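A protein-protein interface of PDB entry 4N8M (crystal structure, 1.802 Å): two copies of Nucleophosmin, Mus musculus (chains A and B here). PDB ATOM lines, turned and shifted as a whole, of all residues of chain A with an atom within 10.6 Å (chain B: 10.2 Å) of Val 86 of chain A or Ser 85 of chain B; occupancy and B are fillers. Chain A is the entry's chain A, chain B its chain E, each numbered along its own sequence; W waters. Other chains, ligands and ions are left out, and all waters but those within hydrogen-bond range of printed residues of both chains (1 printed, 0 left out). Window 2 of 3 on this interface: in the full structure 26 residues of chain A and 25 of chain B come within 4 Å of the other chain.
The side-chain hydroxyl (OG1) of Thr 81 of chain A lies within hydrogen-bond range of the backbone carbonyl oxygen (O) of Leu 52 of chain B, 2.7 Å away.
The backbone carbonyl oxygen (O) of Thr 81 of chain A sits at hydrogen-bond distance from the side-chain hydroxyl (OG1) of Thr 89 of chain B, 2.7 Å away.
The backbone NH (N) of Thr 89 of chain B is in hydrogen-bond range of the side-chain amide oxygen (OE1) of Gln 87 of chain A.
The backbone nitrogen of Pro 88 of chain B lies close to the side-chain amide oxygen of Gln 87 of chain A, 3.4 Å away.
N of Leu 52 of chain B is in hydrogen-bond range of O of Pro 88 of chain B.
The side-chain carboxylate of Asp 58 of chain B is in hydrogen-bond range of the backbone NH of Met 84 of chain B (3.3 Å).
OG of Ser 85 of chain B is in hydrogen-bond range of OD2 of Asp 58 of chain B, at 2.9 Å.
Leu 60 of chain A touches Met 84 of chain B (CD1 to SD, 3.8 Å).
Thr 81 of chain A touches Pro 88 of chain B.
Val 86 of chain A touches Ser 85 of chain B (CG2 to O, 3.7 Å).
Val 86 of chain A touches Val 86 of chain B (CG1 to O, 3.4 Å).
Val 86 of chain A touches Pro 88 of chain B (CG1 to CD, 3.7 Å).
Thr 89 of chain B touches Val 90 of chain A (CB to CG2, 3.96 Å).
Of the printed residues of chain B, Val 86 of chain A touches Ser 85, Val 86 and Pro 88.
Ser 85 of chain B touches just one residue of chain A: Val 86.
No residue of chain B comes within 4 Å of Lys 83 of chain A.
No residue of chain B comes within 4 Å of Ser 85 of chain A.
No residue of chain A comes within 4 Å of Lys 83 of chain B.
Of the printed residues of chain B, Thr 81 of chain A touches Leu 52, Pro 88 and Thr 89.
Printed residues of chain B within 4 Å of Gln 87 of chain A: Pro 88 and Thr 89.
The nearest printed residue of chain A that does not touch Thr 89 of chain B is Leu 82 of chain A (4.7 Å).
Of the 16 printed residues of chain A, 5 touch a printed residue of chain B.
Printed residues of chain A that touch a printed residue of chain B: Leu 60, Thr 81, Val 86, Gln 87 and Val 90.
Of the 17 printed residues of chain B, 6 touch a printed residue of chain A.
Hydrophobic or aromatic side chains of chain B within 4 Å of the printed part of chain A: Met 84 and Pro 88.
Among the printed residues, 10 pairs touch across the chains.
Among the printed residues, no Asp or Glu carboxylate lies within 4 Å of a Lys or Arg side-chain nitrogen of the other chain.
Thr 81 of chain A touches Thr 89 of chain B, but with the chains exchanged Thr 89 of chain A does not touch Thr 81 of chain B (13.7 Å).
Val 86 of chain B touches its own counterpart, Val 86 of chain A.
Val 86 of chain A touches Pro 88 of chain B, but with the chains exchanged Pro 88 of chain A does not touch Val 86 of chain B (8.5 Å).
Gln 87 of chain A touches Pro 88 of chain B, but with the chains exchanged Pro 88 of chain A does not touch Gln 87 of chain B (9.2 Å).
15 positions are printed for both chains.
Water W1 lies within hydrogen-bond range of O of Thr 89 of chain B, NE2 of Gln 87 of chain A and NE2 of Gln 87 of chain B.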
ATOM      1  N   LEU A  52      -4.951 -27.253  -6.016  1.00  0.00           N
ATOM      2  CA  LEU A  52      -5.694 -27.791  -4.873  1.00  0.00           C
ATOM      3  C   LEU A  52      -6.248 -29.172  -5.216  1.00  0.00           C
ATOM      4  O   LEU A  52      -6.692 -29.424  -6.343  1.00  0.00           O
ATOM      5  CB  LEU A  52      -6.809 -26.841  -4.478  1.00  0.00           C
ATOM      6  CG  LEU A  52      -6.312 -25.478  -3.977  1.00  0.00           C
ATOM      7  CD1 LEU A  52      -7.473 -24.579  -3.612  1.00  0.00           C
ATOM      8  CD2 LEU A  52      -5.358 -25.628  -2.801  1.00  0.00           C
ATOM      9  N   LYS A  57     -10.875 -27.787   1.075  1.00  0.00           N
ATOM     10  CA  LYS A  57     -12.055 -26.936   1.241  1.00  0.00           C
ATOM     11  C   LYS A  57     -11.757 -25.545   0.677  1.00  0.00           C
ATOM     12  O   LYS A  57     -10.789 -25.389  -0.072  1.00  0.00           O
ATOM     13  CB  LYS A  57     -12.491 -26.884   2.711  1.00  0.00           C
ATOM     14  CG  LYS A  57     -12.922 -28.242   3.233  1.00  0.00           C
ATOM     15  CD  LYS A  57     -14.050 -28.818   2.393  1.00  0.00           C
ATOM     16  CE  LYS A  57     -14.529 -30.158   2.936  1.00  0.00           C
ATOM     17  NZ  LYS A  57     -13.503 -31.226   2.784  1.00  0.00           N
ATOM     18  N   ASP A  58     -12.571 -24.545   1.021  1.00  0.00           N
ATOM     19  CA  ASP A  58     -12.434 -23.222   0.404  1.00  0.00           C
ATOM     20  C   ASP A  58     -11.632 -22.213   1.247  1.00  0.00           C
ATOM     21  O   ASP A  58     -11.747 -20.996   1.066  1.00  0.00           O
ATOM     22  CB  ASP A  58     -13.815 -22.636   0.046  1.00  0.00           C
ATOM     23  CG  ASP A  58     -13.734 -21.553  -1.046  1.00  0.00           C
ATOM     24  OD1 ASP A  58     -12.806 -21.590  -1.899  1.00  0.00           O
ATOM     25  OD2 ASP A  58     -14.604 -20.660  -1.061  1.00  0.00           O
ATOM     26  N   GLU A  59     -10.816 -22.712   2.164  1.00  0.00           N
ATOM     27  CA  GLU A  59      -9.983 -21.827   2.975  1.00  0.00           C
ATOM     28  C   GLU A  59      -8.741 -21.373   2.200  1.00  0.00           C
ATOM     29  O   GLU A  59      -8.366 -21.989   1.216  1.00  0.00           O
ATOM     30  CB  GLU A  59      -9.612 -22.484   4.319  1.00  0.00           C
ATOM     31  CG  GLU A  59      -8.471 -23.490   4.304  1.00  0.00           C
ATOM     32  CD  GLU A  59      -8.881 -24.894   3.868  1.00  0.00           C
ATOM     33  OE1 GLU A  59      -9.889 -25.044   3.148  1.00  0.00           O
ATOM     34  OE2 GLU A  59      -8.176 -25.857   4.245  1.00  0.00           O
ATOM     35  N   LEU A  60      -8.105 -20.294   2.640  1.00  0.00           N
ATOM     36  CA  LEU A  60      -6.868 -19.863   1.994  1.00  0.00           C
ATOM     37  C   LEU A  60      -5.783 -20.940   2.146  1.00  0.00           C
ATOM     38  O   LEU A  60      -5.600 -21.499   3.233  1.00  0.00           O
ATOM     39  CB  LEU A  60      -6.383 -18.565   2.644  1.00  0.00           C
ATOM     40  CG  LEU A  60      -5.441 -17.704   1.813  1.00  0.00           C
ATOM     41  CD1 LEU A  60      -6.098 -17.372   0.471  1.00  0.00           C
ATOM     42  CD2 LEU A  60      -5.115 -16.437   2.586  1.00  0.00           C
ATOM     43  N   HIS A  61      -5.078 -21.230   1.057  1.00  0.00           N
ATOM     44  CA  HIS A  61      -3.937 -22.138   1.118  1.00  0.00           C
ATOM     45  C   HIS A  61      -2.702 -21.361   0.705  1.00  0.00           C
ATOM     46  O   HIS A  61      -2.703 -20.693  -0.337  1.00  0.00           O
ATOM     47  CB  HIS A  61      -4.104 -23.322   0.160  1.00  0.00           C
ATOM     48  CG  HIS A  61      -5.052 -24.372   0.646  1.00  0.00           C
ATOM     49  ND1 HIS A  61      -6.419 -24.265   0.507  1.00  0.00           N
ATOM     50  CD2 HIS A  61      -4.827 -25.561   1.254  1.00  0.00           C
ATOM     51  CE1 HIS A  61      -6.998 -25.335   1.026  1.00  0.00           C
ATOM     52  NE2 HIS A  61      -6.052 -26.143   1.475  1.00  0.00           N
ATOM     53  N   THR A  81      -0.483 -18.534  -3.302  1.00  0.00           N
ATOM     54  CA  THR A  81      -1.675 -18.470  -2.481  1.00  0.00           C
ATOM     55  C   THR A  81      -2.840 -18.934  -3.344  1.00  0.00           C
ATOM     56  O   THR A  81      -3.081 -18.366  -4.413  1.00  0.00           O
ATOM     57  CB  THR A  81      -1.921 -17.024  -2.024  1.00  0.00           C
ATOM     58  OG1 THR A  81      -0.821 -16.621  -1.193  1.00  0.00           O
ATOM     59  CG2 THR A  81      -3.212 -16.918  -1.230  1.00  0.00           C
ATOM     60  N   LEU A  82      -3.541 -19.973  -2.893  1.00  0.00           N
ATOM     61  CA  LEU A  82      -4.646 -20.558  -3.658  1.00  0.00           C
ATOM     62  C   LEU A  82      -5.935 -20.547  -2.841  1.00  0.00           C
ATOM     63  O   LEU A  82      -5.912 -20.587  -1.609  1.00  0.00           O
ATOM     64  CB  LEU A  82      -4.336 -22.011  -4.033  1.00  0.00           C
ATOM     65  CG  LEU A  82      -3.098 -22.338  -4.885  1.00  0.00           C
ATOM     66  CD1 LEU A  82      -2.910 -23.851  -5.015  1.00  0.00           C
ATOM     67  CD2 LEU A  82      -3.240 -21.748  -6.258  1.00  0.00           C
ATOM     68  N   LYS A  83      -7.063 -20.511  -3.540  1.00  0.00           N
ATOM     69  CA  LYS A  83      -8.371 -20.650  -2.901  1.00  0.00           C
ATOM     70  C   LYS A  83      -9.300 -21.327  -3.896  1.00  0.00           C
ATOM     71  O   LYS A  83      -9.373 -20.934  -5.061  1.00  0.00           O
ATOM     72  CB  LYS A  83      -8.925 -19.288  -2.490  1.00  0.00           C
ATOM     73  CG  LYS A  83     -10.229 -19.358  -1.729  1.00  0.00           C
ATOM     74  CD  LYS A  83     -10.672 -17.943  -1.345  1.00  0.00           C
ATOM     75  CE  LYS A  83     -11.379 -17.899  -0.003  1.00  0.00           C
ATOM     76  NZ  LYS A  83     -12.700 -18.565  -0.061  1.00  0.00           N
ATOM     77  N   MET A  84      -9.996 -22.357  -3.450  1.00  0.00           N
ATOM     78  CA  MET A  84     -10.748 -23.202  -4.390  1.00  0.00           C
ATOM     79  C   MET A  84     -11.758 -22.436  -5.261  1.00  0.00           C
ATOM     80  O   MET A  84     -11.900 -22.708  -6.457  1.00  0.00           O
ATOM     81  CB  MET A  84     -11.482 -24.304  -3.626  1.00  0.00           C
ATOM     82  CG  MET A  84     -12.102 -25.353  -4.551  1.00  0.00           C
ATOM     83  SD  MET A  84     -10.867 -26.362  -5.395  1.00  0.00           S
ATOM     84  CE  MET A  84     -10.361 -27.497  -4.095  1.00  0.00           C
ATOM     85  N   SER A  85     -12.458 -21.475  -4.669  1.00  0.00           N
ATOM     86  CA  SER A  85     -13.533 -20.803  -5.391  1.00  0.00           C
ATOM     87  C   SER A  85     -13.041 -19.635  -6.242  1.00  0.00           C
ATOM     88  O   SER A  85     -13.840 -18.985  -6.914  1.00  0.00           O
ATOM     89  CB  SER A  85     -14.598 -20.309  -4.407  1.00  0.00           C
ATOM     90  OG  SER A  85     -14.016 -19.388  -3.504  1.00  0.00           O
ATOM     91  N   VAL A  86     -11.735 -19.381  -6.205  1.00  0.00           N
ATOM     92  CA  VAL A  86     -11.147 -18.225  -6.873  1.00  0.00           C
ATOM     93  C   VAL A  86     -10.016 -18.610  -7.823  1.00  0.00           C
ATOM     94  O   VAL A  86     -10.001 -18.198  -8.988  1.00  0.00           O
ATOM     95  CB  VAL A  86     -10.589 -17.220  -5.827  1.00  0.00           C
ATOM     96  CG1 VAL A  86      -9.970 -16.025  -6.544  1.00  0.00           C
ATOM     97  CG2 VAL A  86     -11.710 -16.769  -4.869  1.00  0.00           C
ATOM     98  N   GLN A  87      -9.050 -19.371  -7.318  1.00  0.00           N
ATOM     99  CA  GLN A  87      -7.854 -19.741  -8.091  1.00  0.00           C
ATOM    100  C   GLN A  87      -7.314 -21.079  -7.560  1.00  0.00           C
ATOM    101  O   GLN A  87      -6.480 -21.103  -6.666  1.00  0.00           O
ATOM    102  CB  GLN A  87      -6.799 -18.616  -7.957  1.00  0.00           C
ATOM    103  CG  GLN A  87      -5.484 -18.795  -8.727  1.00  0.00           C
ATOM    104  CD  GLN A  87      -4.607 -17.521  -8.734  1.00  0.00           C
ATOM    105  OE1 GLN A  87      -4.670 -16.684  -7.830  1.00  0.00           O
ATOM    106  NE2 GLN A  87      -3.785 -17.384  -9.762  1.00  0.00           N
ATOM    107  N   PRO A  88      -7.826 -22.205  -8.093  1.00  0.00           N
ATOM    108  CA  PRO A  88      -7.419 -23.516  -7.581  1.00  0.00           C
ATOM    109  C   PRO A  88      -6.068 -23.995  -8.108  1.00  0.00           C
ATOM    110  O   PRO A  88      -5.502 -24.877  -7.489  1.00  0.00           O
ATOM    111  CB  PRO A  88      -8.534 -24.454  -8.062  1.00  0.00           C
ATOM    112  CG  PRO A  88      -9.143 -23.763  -9.223  1.00  0.00           C
ATOM    113  CD  PRO A  88      -9.009 -22.290  -8.964  1.00  0.00           C
ATOM    114  N   THR A  89      -5.571 -23.430  -9.205  1.00  0.00           N
ATOM    115  CA  THR A  89      -4.258 -23.815  -9.747  1.00  0.00           C
ATOM    116  C   THR A  89      -3.406 -22.585 -10.057  1.00  0.00           C
ATOM    117  O   THR A  89      -3.905 -21.617 -10.624  1.00  0.00           O
ATOM    118  CB  THR A  89      -4.409 -24.599 -11.080  1.00  0.00           C
ATOM    119  OG1 THR A  89      -5.162 -25.787 -10.853  1.00  0.00           O
ATOM    120  CG2 THR A  89      -3.041 -24.998 -11.653  1.00  0.00           C
ATOM    121  N   VAL A  90      -2.124 -22.626  -9.698  1.00  0.00           N
ATOM    122  CA  VAL A  90      -1.190 -21.579 -10.107  1.00  0.00           C
ATOM    123  C   VAL A  90      -0.077 -22.244 -10.905  1.00  0.00           C
ATOM    124  O   VAL A  90       0.470 -23.271 -10.476  1.00  0.00           O
ATOM    125  CB  VAL A  90      -0.595 -20.856  -8.878  1.00  0.00           C
ATOM    126  CG1 VAL A  90       0.657 -20.070  -9.264  1.00  0.00           C
ATOM    127  CG2 VAL A  90      -1.651 -19.942  -8.235  1.00  0.00           C
ATOM    128  N   LEU B  52      -0.755 -12.781  -2.187  1.00  0.00           N
ATOM    129  CA  LEU B  52      -1.291 -12.172  -0.966  1.00  0.00           C
ATOM    130  C   LEU B  52      -1.064 -13.108   0.211  1.00  0.00           C
ATOM    131  O   LEU B  52      -1.210 -14.321   0.079  1.00  0.00           O
ATOM    132  CB  LEU B  52      -2.784 -11.909  -1.123  1.00  0.00           C
ATOM    133  CG  LEU B  52      -3.119 -10.878  -2.195  1.00  0.00           C
ATOM    134  CD1 LEU B  52      -4.634 -10.660  -2.325  1.00  0.00           C
ATOM    135  CD2 LEU B  52      -2.425  -9.572  -1.870  1.00  0.00           C
ATOM    136  N   GLY B  53      -0.711 -12.543   1.362  1.00  0.00           N
ATOM    137  CA  GLY B  53      -0.496 -13.334   2.559  1.00  0.00           C
ATOM    138  C   GLY B  53      -1.759 -13.499   3.387  1.00  0.00           C
ATOM    139  O   GLY B  53      -2.766 -12.816   3.164  1.00  0.00           O
ATOM    140  N   ALA B  56      -4.213 -10.617   4.765  1.00  0.00           N
ATOM    141  CA  ALA B  56      -4.457  -9.541   3.823  1.00  0.00           C
ATOM    142  C   ALA B  56      -5.968  -9.429   3.680  1.00  0.00           C
ATOM    143  O   ALA B  56      -6.668 -10.447   3.634  1.00  0.00           O
ATOM    144  CB  ALA B  56      -3.811  -9.843   2.475  1.00  0.00           C
ATOM    145  N   LYS B  57      -6.474  -8.202   3.629  1.00  0.00           N
ATOM    146  CA  LYS B  57      -7.910  -7.973   3.472  1.00  0.00           C
ATOM    147  C   LYS B  57      -8.266  -7.942   1.992  1.00  0.00           C
ATOM    148  O   LYS B  57      -7.405  -8.175   1.141  1.00  0.00           O
ATOM    149  CB  LYS B  57      -8.333  -6.670   4.161  1.00  0.00           C
ATOM    150  CG  LYS B  57      -8.038  -6.644   5.657  1.00  0.00           C
ATOM    151  CD  LYS B  57      -8.730  -7.789   6.385  1.00  0.00           C
ATOM    152  CE  LYS B  57      -8.270  -7.866   7.835  1.00  0.00           C
ATOM    153  NZ  LYS B  57      -8.825  -9.044   8.559  1.00  0.00           N
ATOM    154  N   ASP B  58      -9.526  -7.658   1.678  1.00  0.00           N
ATOM    155  CA  ASP B  58      -9.966  -7.740   0.285  1.00  0.00           C
ATOM    156  C   ASP B  58      -9.833  -6.440  -0.513  1.00  0.00           C
ATOM    157  O   ASP B  58     -10.482  -6.280  -1.541  1.00  0.00           O
ATOM    158  CB  ASP B  58     -11.388  -8.310   0.181  1.00  0.00           C
ATOM    159  CG  ASP B  58     -11.681  -8.904  -1.196  1.00  0.00           C
ATOM    160  OD1 ASP B  58     -10.717  -9.304  -1.897  1.00  0.00           O
ATOM    161  OD2 ASP B  58     -12.871  -8.969  -1.581  1.00  0.00           O
ATOM    162  N   GLU B  59      -8.990  -5.518  -0.056  1.00  0.00           N
ATOM    163  CA  GLU B  59      -8.735  -4.305  -0.830  1.00  0.00           C
ATOM    164  C   GLU B  59      -7.753  -4.581  -1.977  1.00  0.00           C
ATOM    165  O   GLU B  59      -7.039  -5.587  -1.977  1.00  0.00           O
ATOM    166  CB  GLU B  59      -8.180  -3.187   0.045  1.00  0.00           C
ATOM    167  CG  GLU B  59      -6.697  -3.315   0.380  1.00  0.00           C
ATOM    168  CD  GLU B  59      -6.423  -4.184   1.601  1.00  0.00           C
ATOM    169  OE1 GLU B  59      -7.237  -5.089   1.885  1.00  0.00           O
ATOM    170  OE2 GLU B  59      -5.391  -3.956   2.278  1.00  0.00           O
ATOM    171  N   LEU B  60      -7.724  -3.673  -2.943  1.00  0.00           N
ATOM    172  CA  LEU B  60      -6.801  -3.777  -4.072  1.00  0.00           C
ATOM    173  C   LEU B  60      -5.361  -3.666  -3.571  1.00  0.00           C
ATOM    174  O   LEU B  60      -5.056  -2.777  -2.773  1.00  0.00           O
ATOM    175  CB  LEU B  60      -7.091  -2.626  -5.033  1.00  0.00           C
ATOM    176  CG  LEU B  60      -6.772  -2.807  -6.504  1.00  0.00           C
ATOM    177  CD1 LEU B  60      -7.501  -4.039  -7.032  1.00  0.00           C
ATOM    178  CD2 LEU B  60      -7.175  -1.550  -7.269  1.00  0.00           C
ATOM    179  N   HIS B  61      -4.486  -4.569  -4.013  1.00  0.00           N
ATOM    180  CA  HIS B  61      -3.058  -4.439  -3.761  1.00  0.00           C
ATOM    181  C   HIS B  61      -2.304  -4.220  -5.063  1.00  0.00           C
ATOM    182  O   HIS B  61      -2.447  -4.985  -6.012  1.00  0.00           O
ATOM    183  CB  HIS B  61      -2.497  -5.704  -3.123  1.00  0.00           C
ATOM    184  CG  HIS B  61      -2.918  -5.889  -1.702  1.00  0.00           C
ATOM    185  ND1 HIS B  61      -4.184  -6.308  -1.354  1.00  0.00           N
ATOM    186  CD2 HIS B  61      -2.249  -5.699  -0.541  1.00  0.00           C
ATOM    187  CE1 HIS B  61      -4.275  -6.372  -0.036  1.00  0.00           C
ATOM    188  NE2 HIS B  61      -3.113  -6.015   0.480  1.00  0.00           N
ATOM    189  N   THR B  81      -1.438  -6.322  -9.926  1.00  0.00           N
ATOM    190  CA  THR B  81      -2.603  -5.885  -9.155  1.00  0.00           C
ATOM    191  C   THR B  81      -3.305  -7.146  -8.671  1.00  0.00           C
ATOM    192  O   THR B  81      -3.658  -8.011  -9.477  1.00  0.00           O
ATOM    193  CB  THR B  81      -3.574  -5.077 -10.026  1.00  0.00           C
ATOM    194  OG1 THR B  81      -2.925  -3.885 -10.473  1.00  0.00           O
ATOM    195  CG2 THR B  81      -4.824  -4.693  -9.239  1.00  0.00           C
ATOM    196  N   LEU B  82      -3.486  -7.263  -7.359  1.00  0.00           N
ATOM    197  CA  LEU B  82      -4.013  -8.484  -6.756  1.00  0.00           C
ATOM    198  C   LEU B  82      -5.212  -8.111  -5.901  1.00  0.00           C
ATOM    199  O   LEU B  82      -5.286  -7.006  -5.371  1.00  0.00           O
ATOM    200  CB  LEU B  82      -2.976  -9.137  -5.834  1.00  0.00           C
ATOM    201  CG  LEU B  82      -1.604  -9.535  -6.385  1.00  0.00           C
ATOM    202  CD1 LEU B  82      -0.747 -10.157  -5.297  1.00  0.00           C
ATOM    203  CD2 LEU B  82      -1.784 -10.522  -7.485  1.00  0.00           C
ATOM    204  N   LYS B  83      -6.141  -9.047  -5.762  1.00  0.00           N
ATOM    205  CA  LYS B  83      -7.303  -8.859  -4.887  1.00  0.00           C
ATOM    206  C   LYS B  83      -7.699 -10.249  -4.423  1.00  0.00           C
ATOM    207  O   LYS B  83      -7.830 -11.165  -5.239  1.00  0.00           O
ATOM    208  CB  LYS B  83      -8.450  -8.197  -5.652  1.00  0.00           C
ATOM    209  CG  LYS B  83      -9.531  -7.582  -4.754  1.00  0.00           C
ATOM    210  CD  LYS B  83     -10.700  -7.066  -5.593  1.00  0.00           C
ATOM    211  CE  LYS B  83     -11.236  -5.744  -5.072  1.00  0.00           C
ATOM    212  NZ  LYS B  83     -11.791  -5.847  -3.702  1.00  0.00           N
ATOM    213  N   MET B  84      -7.874 -10.413  -3.116  1.00  0.00           N
ATOM    214  CA  MET B  84      -8.054 -11.744  -2.527  1.00  0.00           C
ATOM    215  C   MET B  84      -9.226 -12.527  -3.139  1.00  0.00           C
ATOM    216  O   MET B  84      -9.133 -13.741  -3.359  1.00  0.00           O
ATOM    217  CB  MET B  84      -8.242 -11.631  -1.010  1.00  0.00           C
ATOM    218  CG  MET B  84      -8.207 -12.975  -0.312  1.00  0.00           C
ATOM    219  SD  MET B  84      -6.559 -13.699  -0.360  1.00  0.00           S
ATOM    220  CE  MET B  84      -5.715 -12.718   0.883  1.00  0.00           C
ATOM    221  N   SER B  85     -10.316 -11.831  -3.436  1.00  0.00           N
ATOM    222  CA  SER B  85     -11.517 -12.497  -3.918  1.00  0.00           C
ATOM    223  C   SER B  85     -11.531 -12.731  -5.426  1.00  0.00           C
ATOM    224  O   SER B  85     -12.471 -13.324  -5.955  1.00  0.00           O
ATOM    225  CB  SER B  85     -12.764 -11.710  -3.500  1.00  0.00           C
ATOM    226  OG  SER B  85     -12.740 -10.401  -4.050  1.00  0.00           O
ATOM    227  N   VAL B  86     -10.494 -12.262  -6.115  1.00  0.00           N
ATOM    228  CA  VAL B  86     -10.459 -12.316  -7.578  1.00  0.00           C
ATOM    229  C   VAL B  86      -9.181 -12.959  -8.108  1.00  0.00           C
ATOM    230  O   VAL B  86      -9.237 -13.795  -9.013  1.00  0.00           O
ATOM    231  CB  VAL B  86     -10.587 -10.902  -8.192  1.00  0.00           C
ATOM    232  CG1 VAL B  86     -10.507 -10.964  -9.709  1.00  0.00           C
ATOM    233  CG2 VAL B  86     -11.891 -10.222  -7.741  1.00  0.00           C
ATOM    234  N   GLN B  87      -8.037 -12.561  -7.556  1.00  0.00           N
ATOM    235  CA  GLN B  87      -6.744 -13.022  -8.066  1.00  0.00           C
ATOM    236  C   GLN B  87      -5.689 -12.850  -6.978  1.00  0.00           C
ATOM    237  O   GLN B  87      -5.061 -11.794  -6.876  1.00  0.00           O
ATOM    238  CB  GLN B  87      -6.368 -12.234  -9.331  1.00  0.00           C
ATOM    239  CG  GLN B  87      -5.166 -12.798 -10.080  1.00  0.00           C
ATOM    240  CD  GLN B  87      -4.895 -12.099 -11.406  1.00  0.00           C
ATOM    241  OE1 GLN B  87      -5.475 -11.065 -11.716  1.00  0.00           O
ATOM    242  NE2 GLN B  87      -3.995 -12.668 -12.192  1.00  0.00           N
ATOM    243  N   PRO B  88      -5.525 -13.870  -6.118  1.00  0.00           N
ATOM    244  CA  PRO B  88      -4.583 -13.707  -5.001  1.00  0.00           C
ATOM    245  C   PRO B  88      -3.115 -13.951  -5.358  1.00  0.00           C
ATOM    246  O   PRO B  88      -2.274 -13.575  -4.562  1.00  0.00           O
ATOM    247  CB  PRO B  88      -5.067 -14.737  -3.968  1.00  0.00           C
ATOM    248  CG  PRO B  88      -5.820 -15.748  -4.759  1.00  0.00           C
ATOM    249  CD  PRO B  88      -6.462 -14.986  -5.893  1.00  0.00           C
ATOM    250  N   THR B  89      -2.828 -14.548  -6.510  1.00  0.00           N
ATOM    251  CA  THR B  89      -1.459 -14.813  -6.926  1.00  0.00           C
ATOM    252  C   THR B  89      -1.307 -14.468  -8.392  1.00  0.00           C
ATOM    253  O   THR B  89      -2.187 -14.743  -9.213  1.00  0.00           O
ATOM    254  CB  THR B  89      -1.083 -16.309  -6.765  1.00  0.00           C
ATOM    255  OG1 THR B  89      -1.208 -16.689  -5.392  1.00  0.00           O
ATOM    256  CG2 THR B  89       0.366 -16.573  -7.234  1.00  0.00           C
HETATM  257  O   HOH W   1      -3.011 -15.509 -11.847  1.00  0.00           O
